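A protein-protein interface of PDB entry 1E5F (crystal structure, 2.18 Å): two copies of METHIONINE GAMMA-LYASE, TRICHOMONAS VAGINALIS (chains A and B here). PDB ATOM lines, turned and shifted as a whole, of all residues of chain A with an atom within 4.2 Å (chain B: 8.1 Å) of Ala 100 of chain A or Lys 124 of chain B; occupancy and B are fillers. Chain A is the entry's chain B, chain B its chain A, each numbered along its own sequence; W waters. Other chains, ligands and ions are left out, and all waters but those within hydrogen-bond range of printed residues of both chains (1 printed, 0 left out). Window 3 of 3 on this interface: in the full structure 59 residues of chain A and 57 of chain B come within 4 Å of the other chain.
CZ of Phe 125 of chain B touches CD2 of Leu 95 of chain A (3.7 Å).
Leu 98 of chain A touches Phe 125 of chain B (O to CE1, 3.6 Å).
Lys 124 of chain B touches Lys 99 of chain A.
Ala 100 of chain A touches just one residue of chain B: Lys 124 (2.8 Å).
Of chain A, only Leu 95, Thr 96, Leu 98, Lys 99 and Ala 100 come within 4 Å of Lys 124 of chain B.
Lys 99 of chain A touches just one residue of chain B: Lys 124 (3.5 Å).
Printed residues of chain B within 4 Å of Leu 98 of chain A: Lys 124 and Phe 125.
Printed residues of chain B within 4 Å of Phe 125 of chain A: Phe 125 (3.5 Å).
Leu 122 of chain B touches none of the printed residues of chain A.
Val 129 of chain B touches none of the printed residues of chain A.
The nearest residue of chain B that does not touch Ala 100 of chain A is Phe 125 of chain B (4.02 Å).
Phe 125 of chain B touches its own counterpart, Phe 125 of chain A.
The side-chain amino group (NZ) of Lys 124 of chain B is in hydrogen-bond range of the backbone carbonyl oxygen (O) of Leu 95 of chain A (3.0 Å).
The side-chain amino group (NZ) of Lys 124 of chain B sits at hydrogen-bond distance from the backbone carbonyl oxygen (O) of Thr 96 of chain A.
The side-chain amino group of Lys 124 of chain B lies within hydrogen-bond range of the backbone carbonyl oxygen of Leu 98 of chain A, at 3.3 Å.
The backbone carbonyl oxygen of Lys 124 of chain B is in hydrogen-bond range of the backbone NH of Ala 100 of chain A (2.8 Å).
O of Phe 125 of chain B sits close to O of Phe 125 of chain A (3.5 Å).
Water W1 lies within hydrogen-bond range of the backbone carbonyl oxygen of Ala 100 of chain A (3.2 Å) and the backbone carbonyl oxygen of Lys 124 of chain B (3.3 Å).
N of Lys 99 of chain A lies within hydrogen-bond range of OD2 of Asp 102 of chain A, at 3.0 Å.
Among the printed residues, no Asp or Glu carboxylate lies within 4 Å of a Lys or Arg side-chain nitrogen of the other chain.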
ATOM      1  N   LEU A  95      -3.401 -12.912 -18.401  1.00  0.00           N
ATOM      2  CA  LEU A  95      -2.126 -12.671 -19.058  1.00  0.00           C
ATOM      3  C   LEU A  95      -2.404 -11.706 -20.225  1.00  0.00           C
ATOM      4  O   LEU A  95      -1.455 -11.086 -20.666  1.00  0.00           O
ATOM      5  CB  LEU A  95      -1.561 -14.019 -19.561  1.00  0.00           C
ATOM      6  CG  LEU A  95      -1.165 -14.995 -18.507  1.00  0.00           C
ATOM      7  CD1 LEU A  95      -0.816 -16.347 -19.175  1.00  0.00           C
ATOM      8  CD2 LEU A  95       0.037 -14.487 -17.625  1.00  0.00           C
ATOM      9  N   THR A  96      -3.635 -11.436 -20.683  1.00  0.00           N
ATOM     10  CA  THR A  96      -3.775 -10.282 -21.571  1.00  0.00           C
ATOM     11  C   THR A  96      -3.713  -8.962 -20.769  1.00  0.00           C
ATOM     12  O   THR A  96      -3.140  -7.966 -21.280  1.00  0.00           O
ATOM     13  CB  THR A  96      -5.171 -10.265 -22.206  1.00  0.00           C
ATOM     14  OG1 THR A  96      -5.186 -11.512 -22.956  1.00  0.00           O
ATOM     15  CG2 THR A  96      -5.539  -9.072 -23.103  1.00  0.00           C
ATOM     16  N   LEU A  98      -2.490  -8.246 -17.536  1.00  0.00           N
ATOM     17  CA  LEU A  98      -1.331  -7.944 -16.718  1.00  0.00           C
ATOM     18  C   LEU A  98       0.005  -7.877 -17.430  1.00  0.00           C
ATOM     19  O   LEU A  98       0.197  -8.554 -18.450  1.00  0.00           O
ATOM     20  CB  LEU A  98      -1.246  -9.074 -15.670  1.00  0.00           C
ATOM     21  CG  LEU A  98      -2.481  -9.228 -14.804  1.00  0.00           C
ATOM     22  CD1 LEU A  98      -2.442 -10.447 -13.886  1.00  0.00           C
ATOM     23  CD2 LEU A  98      -2.620  -7.926 -13.984  1.00  0.00           C
ATOM     24  N   LYS A  99       0.997  -7.178 -16.862  1.00  0.00           N
ATOM     25  CA  LYS A  99       2.377  -7.117 -17.343  1.00  0.00           C
ATOM     26  C   LYS A  99       3.182  -7.086 -16.039  1.00  0.00           C
ATOM     27  O   LYS A  99       2.594  -6.764 -14.985  1.00  0.00           O
ATOM     28  CB  LYS A  99       2.519  -5.779 -18.081  1.00  0.00           C
ATOM     29  N   ALA A 100       4.444  -7.337 -16.014  1.00  0.00           N
ATOM     30  CA  ALA A 100       5.377  -7.423 -14.931  1.00  0.00           C
ATOM     31  C   ALA A 100       5.277  -6.100 -14.182  1.00  0.00           C
ATOM     32  O   ALA A 100       5.209  -5.155 -14.966  1.00  0.00           O
ATOM     33  CB  ALA A 100       6.802  -7.471 -15.500  1.00  0.00           C
ATOM     34  N   GLY A 101       5.067  -6.002 -12.879  1.00  0.00           N
ATOM     35  CA  GLY A 101       4.944  -4.678 -12.264  1.00  0.00           C
ATOM     36  C   GLY A 101       3.504  -4.456 -11.873  1.00  0.00           C
ATOM     37  O   GLY A 101       3.185  -3.577 -11.036  1.00  0.00           O
ATOM     38  N   ASP A 102       2.495  -5.150 -12.459  1.00  0.00           N
ATOM     39  CA  ASP A 102       1.106  -4.949 -12.042  1.00  0.00           C
ATOM     40  C   ASP A 102       0.853  -5.725 -10.753  1.00  0.00           C
ATOM     41  O   ASP A 102       1.636  -6.579 -10.338  1.00  0.00           O
ATOM     42  CB  ASP A 102       0.149  -5.440 -13.121  1.00  0.00           C
ATOM     43  CG  ASP A 102       0.232  -4.619 -14.387  1.00  0.00           C
ATOM     44  OD1 ASP A 102       0.773  -3.483 -14.284  1.00  0.00           O
ATOM     45  OD2 ASP A 102      -0.363  -4.980 -15.406  1.00  0.00           O
ATOM     46  N   PHE A 125       6.397 -13.929 -13.508  1.00  0.00           N
ATOM     47  CA  PHE A 125       6.414 -13.013 -14.639  1.00  0.00           C
ATOM     48  C   PHE A 125       6.342 -11.559 -14.118  1.00  0.00           C
ATOM     49  O   PHE A 125       6.138 -10.662 -14.898  1.00  0.00           O
ATOM     50  CB  PHE A 125       5.274 -13.337 -15.591  1.00  0.00           C
ATOM     51  CG  PHE A 125       5.502 -14.711 -16.213  1.00  0.00           C
ATOM     52  CD1 PHE A 125       6.632 -15.045 -16.931  1.00  0.00           C
ATOM     53  CD2 PHE A 125       4.475 -15.603 -16.232  1.00  0.00           C
ATOM     54  CE1 PHE A 125       6.678 -16.291 -17.499  1.00  0.00           C
ATOM     55  CE2 PHE A 125       4.531 -16.890 -16.733  1.00  0.00           C
ATOM     56  CZ  PHE A 125       5.655 -17.196 -17.455  1.00  0.00           C
ATOM     57  N   GLY A 126       6.838 -11.406 -12.892  1.00  0.00           N
ATOM     58  CA  GLY A 126       6.965 -10.094 -12.243  1.00  0.00           C
ATOM     59  C   GLY A 126       5.646  -9.519 -11.790  1.00  0.00           C
ATOM     60  O   GLY A 126       5.602  -8.313 -11.428  1.00  0.00           O
ATOM     61  N   ALA B 100      10.754 -13.917 -15.582  1.00  0.00           N
ATOM     62  CA  ALA B 100      11.253 -12.560 -15.632  1.00  0.00           C
ATOM     63  C   ALA B 100      12.780 -12.459 -15.388  1.00  0.00           C
ATOM     64  O   ALA B 100      13.222 -13.045 -14.409  1.00  0.00           O
ATOM     65  CB  ALA B 100      10.729 -11.654 -14.543  1.00  0.00           C
ATOM     66  N   GLY B 101      13.481 -11.745 -16.314  1.00  0.00           N
ATOM     67  CA  GLY B 101      14.923 -11.817 -15.986  1.00  0.00           C
ATOM     68  C   GLY B 101      15.648 -12.812 -16.851  1.00  0.00           C
ATOM     69  O   GLY B 101      16.866 -12.528 -17.109  1.00  0.00           O
ATOM     70  N   LEU B 117       4.431 -13.196 -30.039  1.00  0.00           N
ATOM     71  CA  LEU B 117       4.480 -13.754 -28.650  1.00  0.00           C
ATOM     72  C   LEU B 117       5.856 -13.340 -28.006  1.00  0.00           C
ATOM     73  O   LEU B 117       5.931 -12.959 -26.896  1.00  0.00           O
ATOM     74  CB  LEU B 117       4.527 -15.302 -28.693  1.00  0.00           C
ATOM     75  CG  LEU B 117       4.820 -16.077 -27.445  1.00  0.00           C
ATOM     76  CD1 LEU B 117       3.725 -15.887 -26.305  1.00  0.00           C
ATOM     77  CD2 LEU B 117       4.904 -17.566 -27.727  1.00  0.00           C
ATOM     78  N   PHE B 118       6.864 -13.655 -28.791  1.00  0.00           N
ATOM     79  CA  PHE B 118       8.224 -13.381 -28.325  1.00  0.00           C
ATOM     80  C   PHE B 118       8.563 -11.928 -28.255  1.00  0.00           C
ATOM     81  O   PHE B 118       8.851 -11.338 -27.151  1.00  0.00           O
ATOM     82  CB  PHE B 118       9.264 -14.068 -29.183  1.00  0.00           C
ATOM     83  CG  PHE B 118       9.498 -15.561 -29.312  1.00  0.00           C
ATOM     84  CD1 PHE B 118       8.714 -16.386 -28.510  1.00  0.00           C
ATOM     85  CD2 PHE B 118      10.427 -16.104 -30.144  1.00  0.00           C
ATOM     86  CE1 PHE B 118       8.927 -17.759 -28.591  1.00  0.00           C
ATOM     87  CE2 PHE B 118      10.674 -17.510 -30.277  1.00  0.00           C
ATOM     88  CZ  PHE B 118       9.855 -18.296 -29.464  1.00  0.00           C
ATOM     89  N   GLU B 119       8.078 -10.988 -29.095  1.00  0.00           N
ATOM     90  CA  GLU B 119       8.484  -9.622 -29.114  1.00  0.00           C
ATOM     91  C   GLU B 119       7.675  -8.841 -28.095  1.00  0.00           C
ATOM     92  O   GLU B 119       8.083  -7.911 -27.488  1.00  0.00           O
ATOM     93  CB  GLU B 119       8.243  -8.996 -30.518  1.00  0.00           C
ATOM     94  CG  GLU B 119       8.698  -7.541 -30.519  1.00  0.00           C
ATOM     95  CD  GLU B 119       8.733  -6.966 -31.922  1.00  0.00           C
ATOM     96  OE1 GLU B 119       8.370  -7.594 -32.926  1.00  0.00           O
ATOM     97  OE2 GLU B 119       9.076  -5.794 -32.107  1.00  0.00           O
ATOM     98  N   HIS B 120       6.370  -9.135 -28.022  1.00  0.00           N
ATOM     99  CA  HIS B 120       5.417  -8.472 -27.204  1.00  0.00           C
ATOM    100  C   HIS B 120       5.038  -9.115 -25.882  1.00  0.00           C
ATOM    101  O   HIS B 120       5.150  -8.500 -24.830  1.00  0.00           O
ATOM    102  CB  HIS B 120       4.132  -8.259 -28.040  1.00  0.00           C
ATOM    103  CG  HIS B 120       4.476  -7.551 -29.326  1.00  0.00           C
ATOM    104  ND1 HIS B 120       5.205  -6.377 -29.146  1.00  0.00           N
ATOM    105  CD2 HIS B 120       4.235  -7.627 -30.638  1.00  0.00           C
ATOM    106  CE1 HIS B 120       5.396  -5.788 -30.302  1.00  0.00           C
ATOM    107  NE2 HIS B 120       4.819  -6.524 -31.224  1.00  0.00           N
ATOM    108  N   ALA B 121       4.654 -10.390 -25.939  1.00  0.00           N
ATOM    109  CA  ALA B 121       4.254 -11.049 -24.687  1.00  0.00           C
ATOM    110  C   ALA B 121       5.350 -11.232 -23.676  1.00  0.00           C
ATOM    111  O   ALA B 121       5.393 -11.003 -22.502  1.00  0.00           O
ATOM    112  CB  ALA B 121       3.574 -12.412 -24.920  1.00  0.00           C
ATOM    113  N   LEU B 122       6.404 -11.944 -24.188  1.00  0.00           N
ATOM    114  CA  LEU B 122       7.568 -12.305 -23.385  1.00  0.00           C
ATOM    115  C   LEU B 122       8.128 -11.025 -22.699  1.00  0.00           C
ATOM    116  O   LEU B 122       8.473 -11.147 -21.540  1.00  0.00           O
ATOM    117  CB  LEU B 122       8.621 -13.160 -24.150  1.00  0.00           C
ATOM    118  CG  LEU B 122       8.278 -14.558 -24.660  1.00  0.00           C
ATOM    119  CD1 LEU B 122       9.527 -15.282 -25.140  1.00  0.00           C
ATOM    120  CD2 LEU B 122       7.564 -15.401 -23.612  1.00  0.00           C
ATOM    121  N   THR B 123       8.259  -9.990 -23.502  1.00  0.00           N
ATOM    122  CA  THR B 123       8.870  -8.789 -22.999  1.00  0.00           C
ATOM    123  C   THR B 123       8.045  -8.025 -22.002  1.00  0.00           C
ATOM    124  O   THR B 123       8.724  -7.543 -21.096  1.00  0.00           O
ATOM    125  CB  THR B 123       9.259  -7.849 -24.151  1.00  0.00           C
ATOM    126  OG1 THR B 123       8.204  -7.502 -24.985  1.00  0.00           O
ATOM    127  CG2 THR B 123      10.420  -8.534 -24.875  1.00  0.00           C
ATOM    128  N   LYS B 124       6.732  -8.124 -21.939  1.00  0.00           N
ATOM    129  CA  LYS B 124       6.013  -7.487 -20.851  1.00  0.00           C
ATOM    130  C   LYS B 124       6.106  -8.307 -19.577  1.00  0.00           C
ATOM    131  O   LYS B 124       5.553  -7.775 -18.578  1.00  0.00           O
ATOM    132  CB  LYS B 124       4.552  -7.162 -21.183  1.00  0.00           C
ATOM    133  CG  LYS B 124       3.730  -8.419 -21.486  1.00  0.00           C
ATOM    134  CD  LYS B 124       2.273  -7.966 -21.611  1.00  0.00           C
ATOM    135  CE  LYS B 124       1.337  -9.194 -21.561  1.00  0.00           C
ATOM    136  NZ  LYS B 124      -0.021  -8.694 -21.783  1.00  0.00           N
ATOM    137  N   PHE B 125       6.548  -9.487 -19.589  1.00  0.00           N
ATOM    138  CA  PHE B 125       6.750 -10.444 -18.514  1.00  0.00           C
ATOM    139  C   PHE B 125       8.129 -10.360 -17.968  1.00  0.00           C
ATOM    140  O   PHE B 125       8.583 -11.300 -17.307  1.00  0.00           O
ATOM    141  CB  PHE B 125       6.358 -11.893 -19.047  1.00  0.00           C
ATOM    142  CG  PHE B 125       4.818 -11.909 -19.180  1.00  0.00           C
ATOM    143  CD1 PHE B 125       3.934 -11.138 -18.411  1.00  0.00           C
ATOM    144  CD2 PHE B 125       4.257 -12.765 -20.143  1.00  0.00           C
ATOM    145  CE1 PHE B 125       2.562 -11.218 -18.567  1.00  0.00           C
ATOM    146  CE2 PHE B 125       2.884 -12.853 -20.275  1.00  0.00           C
ATOM    147  CZ  PHE B 125       2.008 -12.021 -19.553  1.00  0.00           C
ATOM    148  N   GLY B 126       8.972  -9.412 -18.477  1.00  0.00           N
ATOM    149  CA  GLY B 126      10.305  -9.141 -17.951  1.00  0.00           C
ATOM    150  C   GLY B 126      11.373 -10.065 -18.588  1.00  0.00           C
ATOM    151  O   GLY B 126      12.372 -10.398 -17.922  1.00  0.00           O
ATOM    152  N   ILE B 127      10.997 -10.756 -19.694  1.00  0.00           N
ATOM    153  CA  ILE B 127      11.966 -11.658 -20.303  1.00  0.00           C
ATOM    154  C   ILE B 127      12.748 -10.805 -21.271  1.00  0.00           C
ATOM    155  O   ILE B 127      12.029 -10.068 -21.950  1.00  0.00           O
ATOM    156  CB  ILE B 127      11.295 -12.896 -20.978  1.00  0.00           C
ATOM    157  CG1 ILE B 127      10.855 -13.826 -19.804  1.00  0.00           C
ATOM    158  CG2 ILE B 127      12.188 -13.746 -21.813  1.00  0.00           C
ATOM    159  CD1 ILE B 127       9.671 -14.627 -20.287  1.00  0.00           C
ATOM    160  N   GLN B 128      14.068 -10.991 -21.434  1.00  0.00           N
ATOM    161  CA  GLN B 128      14.687 -10.285 -22.558  1.00  0.00           C
ATOM    162  C   GLN B 128      14.751 -11.120 -23.830  1.00  0.00           C
ATOM    163  O   GLN B 128      15.019 -12.287 -23.781  1.00  0.00           O
ATOM    164  CB  GLN B 128      16.102  -9.817 -22.163  1.00  0.00           C
ATOM    165  CG  GLN B 128      16.256  -9.403 -20.720  1.00  0.00           C
ATOM    166  CD  GLN B 128      17.680  -9.408 -20.197  1.00  0.00           C
ATOM    167  OE1 GLN B 128      17.988  -9.497 -18.995  1.00  0.00           O
ATOM    168  NE2 GLN B 128      18.732  -9.395 -20.936  1.00  0.00           N
ATOM    169  N   VAL B 129      14.505 -10.539 -25.004  1.00  0.00           N
ATOM    170  CA  VAL B 129      14.519 -11.250 -26.224  1.00  0.00           C
ATOM    171  C   VAL B 129      15.405 -10.593 -27.298  1.00  0.00           C
ATOM    172  O   VAL B 129      15.166  -9.428 -27.586  1.00  0.00           O
ATOM    173  CB  VAL B 129      13.032 -11.219 -26.752  1.00  0.00           C
ATOM    174  CG1 VAL B 129      12.857 -11.911 -28.060  1.00  0.00           C
ATOM    175  CG2 VAL B 129      12.127 -11.936 -25.756  1.00  0.00           C
HETATM  176  O   HOH W   1       6.437  -4.689 -17.933  1.00  0.00           O
